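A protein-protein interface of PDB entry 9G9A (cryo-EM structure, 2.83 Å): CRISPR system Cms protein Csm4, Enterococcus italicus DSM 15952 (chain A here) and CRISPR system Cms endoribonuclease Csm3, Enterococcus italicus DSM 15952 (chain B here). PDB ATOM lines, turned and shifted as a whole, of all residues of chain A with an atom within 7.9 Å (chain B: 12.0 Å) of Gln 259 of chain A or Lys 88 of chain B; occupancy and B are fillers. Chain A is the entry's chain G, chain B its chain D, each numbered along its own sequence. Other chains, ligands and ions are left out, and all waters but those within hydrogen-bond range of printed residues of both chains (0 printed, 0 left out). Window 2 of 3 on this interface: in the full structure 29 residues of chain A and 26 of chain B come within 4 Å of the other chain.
The backbone NH (N) of Gly 89 of chain B sits at hydrogen-bond distance from the backbone carbonyl oxygen (O) of Asp 258 of chain A (2.7 Å).
OG of Ser 85 of chain B lies close to N of Gln 87 of chain B. The side-chain hydroxyl of Ser 253 of chain A sits close to the backbone NH of Tyr 256 of chain A, at 3.4 Å.
O of Ser 253 of chain A touches CG2 of Ile 91 of chain B (3.7 Å). Ala 257 of chain A touches Ile 91 of chain B. Asp 258 of chain A touches Gln 87 of chain B (O to O, 3.9 Å). Lys 88 of chain B touches Asp 258 of chain A (CA to O, 3.4 Å). Asp 258 of chain A touches Ile 91 of chain B (O to CD1, 3.7 Å). OE1 of Gln 259 of chain A touches CE of Lys 88 of chain B (3.7 Å). CD2 of Leu 260 of chain A touches CD1 of Ile 91 of chain B, 3.8 Å away.
Gln 259 of chain A touches just one residue of chain B: Lys 88 (3.7 Å). No residue of chain B comes within 4 Å of Val 251 of chain A. Of chain B, only Gln 87 (3.9 Å), Lys 88 (3.4 Å), Gly 89 (2.7 Å) and Ile 91 (3.7 Å) come within 4 Å of Asp 258 of chain A. Of chain B, only Ile 91 (3.8 Å) comes within 4 Å of Leu 260 of chain A. No residue of chain B comes within 4 Å of Val 261 of chain A. Of the printed residues of chain A, Gln 87 of chain B touches Asp 258 (3.9 Å). Of the printed residues of chain A, Ile 91 of chain B touches Ser 253, Ala 257, Asp 258 and Leu 260. Of the printed residues of chain B, Ser 253 of chain A touches Ile 91. Ser 85 of chain B touches none of the printed residues of chain A. Ala 90 of chain B touches none of the printed residues of chain A. The nearest residue of chain B that does not touch Gln 259 of chain A is Gly 89 of chain B (4.5 Å). The nearest residue of chain A that does not touch Lys 88 of chain B is Leu 260 of chain A (6.3 Å).
Hydrophobic or aromatic side chains of chain B that line the printed part of chain A: Ile 91. Along chain B the printed residues that touch a printed residue of chain A span positions 87 to 91. Hydrophobic or aromatic side chains of chain A that line the printed part of chain B: Leu 260. Among the printed residues, 8 pairs touch across the chains.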
ATOM      1  N   PHE A 250     -17.858  20.356  -9.369  1.00  0.00           N
ATOM      2  CA  PHE A 250     -17.985  18.925  -9.598  1.00  0.00           C
ATOM      3  C   PHE A 250     -19.354  18.623 -10.192  1.00  0.00           C
ATOM      4  O   PHE A 250     -20.314  19.366  -9.974  1.00  0.00           O
ATOM      5  CB  PHE A 250     -17.804  18.142  -8.297  1.00  0.00           C
ATOM      6  CG  PHE A 250     -16.392  18.116  -7.794  1.00  0.00           C
ATOM      7  CD1 PHE A 250     -15.823  19.239  -7.221  1.00  0.00           C
ATOM      8  CD2 PHE A 250     -15.639  16.958  -7.878  1.00  0.00           C
ATOM      9  CE1 PHE A 250     -14.527  19.211  -6.753  1.00  0.00           C
ATOM     10  CE2 PHE A 250     -14.342  16.925  -7.409  1.00  0.00           C
ATOM     11  CZ  PHE A 250     -13.785  18.053  -6.846  1.00  0.00           C
ATOM     12  N   VAL A 251     -19.437  17.527 -10.945  1.00  0.00           N
ATOM     13  CA  VAL A 251     -20.712  17.113 -11.517  1.00  0.00           C
ATOM     14  C   VAL A 251     -21.547  16.429 -10.446  1.00  0.00           C
ATOM     15  O   VAL A 251     -21.092  15.482  -9.790  1.00  0.00           O
ATOM     16  CB  VAL A 251     -20.487  16.189 -12.722  1.00  0.00           C
ATOM     17  CG1 VAL A 251     -21.818  15.739 -13.296  1.00  0.00           C
ATOM     18  CG2 VAL A 251     -19.663  16.894 -13.779  1.00  0.00           C
ATOM     19  N   SER A 253     -24.598  14.267 -10.120  1.00  0.00           N
ATOM     20  CA  SER A 253     -25.588  13.388 -10.724  1.00  0.00           C
ATOM     21  C   SER A 253     -25.283  11.959 -10.309  1.00  0.00           C
ATOM     22  O   SER A 253     -24.182  11.647  -9.850  1.00  0.00           O
ATOM     23  CB  SER A 253     -25.605  13.518 -12.249  1.00  0.00           C
ATOM     24  OG  SER A 253     -24.308  13.351 -12.779  1.00  0.00           O
ATOM     25  N   TYR A 256     -23.479  10.323 -14.184  1.00  0.00           N
ATOM     26  CA  TYR A 256     -22.401  10.861 -15.012  1.00  0.00           C
ATOM     27  C   TYR A 256     -21.204   9.918 -15.039  1.00  0.00           C
ATOM     28  O   TYR A 256     -20.639   9.644 -16.103  1.00  0.00           O
ATOM     29  CB  TYR A 256     -21.985  12.241 -14.507  1.00  0.00           C
ATOM     30  CG  TYR A 256     -21.059  12.979 -15.446  1.00  0.00           C
ATOM     31  CD1 TYR A 256     -21.543  13.557 -16.611  1.00  0.00           C
ATOM     32  CD2 TYR A 256     -19.706  13.101 -15.169  1.00  0.00           C
ATOM     33  CE1 TYR A 256     -20.703  14.232 -17.474  1.00  0.00           C
ATOM     34  CE2 TYR A 256     -18.861  13.775 -16.027  1.00  0.00           C
ATOM     35  CZ  TYR A 256     -19.363  14.338 -17.178  1.00  0.00           C
ATOM     36  OH  TYR A 256     -18.525  15.013 -18.035  1.00  0.00           O
ATOM     37  N   ALA A 257     -20.804   9.414 -13.876  1.00  0.00           N
ATOM     38  CA  ALA A 257     -19.650   8.531 -13.781  1.00  0.00           C
ATOM     39  C   ALA A 257     -19.744   7.753 -12.476  1.00  0.00           C
ATOM     40  O   ALA A 257     -20.539   8.077 -11.591  1.00  0.00           O
ATOM     41  CB  ALA A 257     -18.336   9.314 -13.863  1.00  0.00           C
ATOM     42  N   ASP A 258     -18.922   6.706 -12.376  1.00  0.00           N
ATOM     43  CA  ASP A 258     -18.873   5.924 -11.145  1.00  0.00           C
ATOM     44  C   ASP A 258     -18.368   6.764  -9.981  1.00  0.00           C
ATOM     45  O   ASP A 258     -18.906   6.688  -8.870  1.00  0.00           O
ATOM     46  CB  ASP A 258     -17.992   4.691 -11.344  1.00  0.00           C
ATOM     47  CG  ASP A 258     -18.509   3.776 -12.436  1.00  0.00           C
ATOM     48  OD1 ASP A 258     -19.742   3.711 -12.622  1.00  0.00           O
ATOM     49  OD2 ASP A 258     -17.683   3.125 -13.108  1.00  0.00           O
ATOM     50  N   GLN A 259     -17.342   7.574 -10.216  1.00  0.00           N
ATOM     51  CA  GLN A 259     -16.788   8.460  -9.206  1.00  0.00           C
ATOM     52  C   GLN A 259     -17.056   9.911  -9.587  1.00  0.00           C
ATOM     53  O   GLN A 259     -17.215  10.244 -10.764  1.00  0.00           O
ATOM     54  CB  GLN A 259     -15.281   8.237  -9.030  1.00  0.00           C
ATOM     55  CG  GLN A 259     -14.426   8.716 -10.196  1.00  0.00           C
ATOM     56  CD  GLN A 259     -14.505   7.800 -11.402  1.00  0.00           C
ATOM     57  OE1 GLN A 259     -14.472   6.578 -11.269  1.00  0.00           O
ATOM     58  NE2 GLN A 259     -14.612   8.389 -12.586  1.00  0.00           N
ATOM     59  N   LEU A 260     -17.114  10.769  -8.572  1.00  0.00           N
ATOM     60  CA  LEU A 260     -17.370  12.185  -8.796  1.00  0.00           C
ATOM     61  C   LEU A 260     -16.179  12.837  -9.486  1.00  0.00           C
ATOM     62  O   LEU A 260     -15.029  12.646  -9.079  1.00  0.00           O
ATOM     63  CB  LEU A 260     -17.663  12.879  -7.470  1.00  0.00           C
ATOM     64  CG  LEU A 260     -18.902  12.369  -6.734  1.00  0.00           C
ATOM     65  CD1 LEU A 260     -18.810  12.701  -5.262  1.00  0.00           C
ATOM     66  CD2 LEU A 260     -20.162  12.962  -7.339  1.00  0.00           C
ATOM     67  N   VAL A 261     -16.457  13.615 -10.534  1.00  0.00           N
ATOM     68  CA  VAL A 261     -15.425  14.275 -11.319  1.00  0.00           C
ATOM     69  C   VAL A 261     -15.815  15.732 -11.529  1.00  0.00           C
ATOM     70  O   VAL A 261     -16.988  16.105 -11.464  1.00  0.00           O
ATOM     71  CB  VAL A 261     -15.192  13.581 -12.678  1.00  0.00           C
ATOM     72  CG1 VAL A 261     -14.563  12.214 -12.475  1.00  0.00           C
ATOM     73  CG2 VAL A 261     -16.498  13.461 -13.437  1.00  0.00           C
ATOM     74  N   LYS A 262     -14.804  16.558 -11.788  1.00  0.00           N
ATOM     75  CA  LYS A 262     -15.017  17.981 -11.993  1.00  0.00           C
ATOM     76  C   LYS A 262     -15.441  18.269 -13.427  1.00  0.00           C
ATOM     77  O   LYS A 262     -15.127  17.519 -14.355  1.00  0.00           O
ATOM     78  CB  LYS A 262     -13.748  18.770 -11.671  1.00  0.00           C
ATOM     79  CG  LYS A 262     -13.195  18.528 -10.283  1.00  0.00           C
ATOM     80  CD  LYS A 262     -12.114  19.534  -9.937  1.00  0.00           C
ATOM     81  CE  LYS A 262     -12.661  20.951  -9.945  1.00  0.00           C
ATOM     82  NZ  LYS A 262     -11.618  21.952  -9.588  1.00  0.00           N
ATOM     83  N   ASN A 289     -16.409  13.661 -21.663  1.00  0.00           N
ATOM     84  CA  ASN A 289     -16.481  12.202 -21.719  1.00  0.00           C
ATOM     85  C   ASN A 289     -17.301  11.648 -20.554  1.00  0.00           C
ATOM     86  O   ASN A 289     -16.818  10.885 -19.715  1.00  0.00           O
ATOM     87  CB  ASN A 289     -15.080  11.587 -21.754  1.00  0.00           C
ATOM     88  CG  ASN A 289     -14.319  11.950 -23.012  1.00  0.00           C
ATOM     89  OD1 ASN A 289     -14.735  12.823 -23.772  1.00  0.00           O
ATOM     90  ND2 ASN A 289     -13.195  11.281 -23.237  1.00  0.00           N
ATOM     91  N   ARG A 291     -21.498  10.270 -19.286  1.00  0.00           N
ATOM     92  CA  ARG A 291     -22.655   9.525 -19.768  1.00  0.00           C
ATOM     93  C   ARG A 291     -23.726  10.463 -20.309  1.00  0.00           C
ATOM     94  O   ARG A 291     -24.428  10.127 -21.269  1.00  0.00           O
ATOM     95  CB  ARG A 291     -23.208   8.640 -18.652  1.00  0.00           C
ATOM     96  CG  ARG A 291     -23.987   7.436 -19.149  1.00  0.00           C
ATOM     97  CD  ARG A 291     -24.036   6.326 -18.106  1.00  0.00           C
ATOM     98  NE  ARG A 291     -22.704   5.861 -17.736  1.00  0.00           N
ATOM     99  CZ  ARG A 291     -22.164   6.005 -16.533  1.00  0.00           C
ATOM    100  NH1 ARG A 291     -22.831   6.564 -15.539  1.00  0.00           N
ATOM    101  NH2 ARG A 291     -20.927   5.569 -16.320  1.00  0.00           N
ATOM    102  N   ARG B  56     -28.817   8.306  11.468  1.00  0.00           N
ATOM    103  CA  ARG B  56     -28.035   7.380  10.660  1.00  0.00           C
ATOM    104  C   ARG B  56     -27.261   6.404  11.535  1.00  0.00           C
ATOM    105  O   ARG B  56     -27.197   5.208  11.234  1.00  0.00           O
ATOM    106  CB  ARG B  56     -27.083   8.157   9.752  1.00  0.00           C
ATOM    107  CG  ARG B  56     -26.216   7.283   8.863  1.00  0.00           C
ATOM    108  CD  ARG B  56     -25.061   8.077   8.276  1.00  0.00           C
ATOM    109  NE  ARG B  56     -24.266   7.281   7.349  1.00  0.00           N
ATOM    110  CZ  ARG B  56     -24.335   7.377   6.029  1.00  0.00           C
ATOM    111  NH1 ARG B  56     -25.147   8.238   5.440  1.00  0.00           N
ATOM    112  NH2 ARG B  56     -23.566   6.595   5.280  1.00  0.00           N
ATOM    113  N   ASP B  75     -21.805   0.995   4.177  1.00  0.00           N
ATOM    114  CA  ASP B  75     -22.881   0.591   5.074  1.00  0.00           C
ATOM    115  C   ASP B  75     -23.965  -0.193   4.343  1.00  0.00           C
ATOM    116  O   ASP B  75     -23.811  -0.544   3.173  1.00  0.00           O
ATOM    117  CB  ASP B  75     -23.495   1.814   5.759  1.00  0.00           C
ATOM    118  CG  ASP B  75     -22.626   2.352   6.878  1.00  0.00           C
ATOM    119  OD1 ASP B  75     -21.611   1.704   7.207  1.00  0.00           O
ATOM    120  OD2 ASP B  75     -22.959   3.421   7.429  1.00  0.00           O
ATOM    121  N   LEU B  80     -27.511   3.967   3.118  1.00  0.00           N
ATOM    122  CA  LEU B  80     -27.083   4.779   1.986  1.00  0.00           C
ATOM    123  C   LEU B  80     -28.272   5.282   1.181  1.00  0.00           C
ATOM    124  O   LEU B  80     -28.226   6.389   0.632  1.00  0.00           O
ATOM    125  CB  LEU B  80     -26.136   3.978   1.095  1.00  0.00           C
ATOM    126  CG  LEU B  80     -24.942   3.323   1.793  1.00  0.00           C
ATOM    127  CD1 LEU B  80     -24.042   2.640   0.778  1.00  0.00           C
ATOM    128  CD2 LEU B  80     -24.163   4.338   2.612  1.00  0.00           C
ATOM    129  N   GLY B  84     -28.036   9.018   1.851  1.00  0.00           N
ATOM    130  CA  GLY B  84     -27.207   9.396   0.728  1.00  0.00           C
ATOM    131  C   GLY B  84     -25.845   8.725   0.773  1.00  0.00           C
ATOM    132  O   GLY B  84     -25.293   8.440   1.844  1.00  0.00           O
ATOM    133  N   SER B  85     -25.292   8.471  -0.411  1.00  0.00           N
ATOM    134  CA  SER B  85     -23.993   7.829  -0.532  1.00  0.00           C
ATOM    135  C   SER B  85     -23.240   8.404  -1.721  1.00  0.00           C
ATOM    136  O   SER B  85     -23.821   8.659  -2.777  1.00  0.00           O
ATOM    137  CB  SER B  85     -24.125   6.312  -0.696  1.00  0.00           C
ATOM    138  OG  SER B  85     -22.861   5.713  -0.907  1.00  0.00           O
ATOM    139  N   SER B  86     -21.928   8.580  -1.544  1.00  0.00           N
ATOM    140  CA  SER B  86     -21.057   9.078  -2.603  1.00  0.00           C
ATOM    141  C   SER B  86     -19.970   8.070  -2.967  1.00  0.00           C
ATOM    142  O   SER B  86     -18.941   8.455  -3.529  1.00  0.00           O
ATOM    143  CB  SER B  86     -20.426  10.413  -2.200  1.00  0.00           C
ATOM    144  OG  SER B  86     -19.677  10.285  -1.005  1.00  0.00           O
ATOM    145  N   GLN B  87     -20.179   6.792  -2.657  1.00  0.00           N
ATOM    146  CA  GLN B  87     -19.183   5.771  -2.948  1.00  0.00           C
ATOM    147  C   GLN B  87     -19.037   5.566  -4.451  1.00  0.00           C
ATOM    148  O   GLN B  87     -19.981   5.754  -5.222  1.00  0.00           O
ATOM    149  CB  GLN B  87     -19.561   4.451  -2.275  1.00  0.00           C
ATOM    150  CG  GLN B  87     -19.769   4.559  -0.773  1.00  0.00           C
ATOM    151  CD  GLN B  87     -18.527   5.024  -0.040  1.00  0.00           C
ATOM    152  OE1 GLN B  87     -17.406   4.674  -0.410  1.00  0.00           O
ATOM    153  NE2 GLN B  87     -18.720   5.823   1.002  1.00  0.00           N
ATOM    154  N   LYS B  88     -17.831   5.175  -4.861  1.00  0.00           N
ATOM    155  CA  LYS B  88     -17.540   4.965  -6.273  1.00  0.00           C
ATOM    156  C   LYS B  88     -18.441   3.881  -6.848  1.00  0.00           C
ATOM    157  O   LYS B  88     -18.409   2.731  -6.401  1.00  0.00           O
ATOM    158  CB  LYS B  88     -16.071   4.586  -6.451  1.00  0.00           C
ATOM    159  CG  LYS B  88     -15.688   4.223  -7.874  1.00  0.00           C
ATOM    160  CD  LYS B  88     -14.234   3.794  -7.958  1.00  0.00           C
ATOM    161  CE  LYS B  88     -13.857   3.402  -9.376  1.00  0.00           C
ATOM    162  NZ  LYS B  88     -12.437   2.970  -9.468  1.00  0.00           N
ATOM    163  N   GLY B  89     -19.251   4.254  -7.838  1.00  0.00           N
ATOM    164  CA  GLY B  89     -20.185   3.339  -8.453  1.00  0.00           C
ATOM    165  C   GLY B  89     -21.491   3.157  -7.715  1.00  0.00           C
ATOM    166  O   GLY B  89     -22.360   2.425  -8.204  1.00  0.00           O
ATOM    167  N   ALA B  90     -21.666   3.795  -6.560  1.00  0.00           N
ATOM    168  CA  ALA B  90     -22.869   3.665  -5.746  1.00  0.00           C
ATOM    169  C   ALA B  90     -23.344   5.033  -5.278  1.00  0.00           C
ATOM    170  O   ALA B  90     -23.651   5.248  -4.103  1.00  0.00           O
ATOM    171  CB  ALA B  90     -22.624   2.739  -4.558  1.00  0.00           C
ATOM    172  N   ILE B  91     -23.408   5.984  -6.205  1.00  0.00           N
ATOM    173  CA  ILE B  91     -23.843   7.341  -5.893  1.00  0.00           C
ATOM    174  C   ILE B  91     -25.361   7.329  -5.747  1.00  0.00           C
ATOM    175  O   ILE B  91     -26.086   7.113  -6.720  1.00  0.00           O
ATOM    176  CB  ILE B  91     -23.397   8.339  -6.967  1.00  0.00           C
ATOM    177  CG1 ILE B  91     -21.869   8.426  -7.016  1.00  0.00           C
ATOM    178  CG2 ILE B  91     -24.006   9.708  -6.711  1.00  0.00           C
ATOM    179  CD1 ILE B  91     -21.348   9.408  -8.038  1.00  0.00           C
ATOM    180  N   GLN B  92     -25.843   7.562  -4.529  1.00  0.00           N
ATOM    181  CA  GLN B  92     -27.267   7.588  -4.231  1.00  0.00           C
ATOM    182  C   GLN B  92     -27.622   8.920  -3.590  1.00  0.00           C
ATOM    183  O   GLN B  92     -26.976   9.340  -2.623  1.00  0.00           O
ATOM    184  CB  GLN B  92     -27.662   6.435  -3.304  1.00  0.00           C
ATOM    185  CG  GLN B  92     -27.284   5.061  -3.823  1.00  0.00           C
ATOM    186  CD  GLN B  92     -27.874   3.943  -2.988  1.00  0.00           C
ATOM    187  OE1 GLN B  92     -27.216   2.940  -2.718  1.00  0.00           O
ATOM    188  NE2 GLN B  92     -29.127   4.108  -2.582  1.00  0.00           N
ATOM    189  N   SER B  93     -28.644   9.578  -4.131  1.00  0.00           N
ATOM    190  CA  SER B  93     -29.119  10.832  -3.563  1.00  0.00           C
ATOM    191  C   SER B  93     -29.817  10.579  -2.233  1.00  0.00           C
ATOM    192  O   SER B  93     -30.549   9.599  -2.074  1.00  0.00           O
ATOM    193  CB  SER B  93     -30.071  11.527  -4.535  1.00  0.00           C
ATOM    194  OG  SER B  93     -30.527  12.760  -4.008  1.00  0.00           O
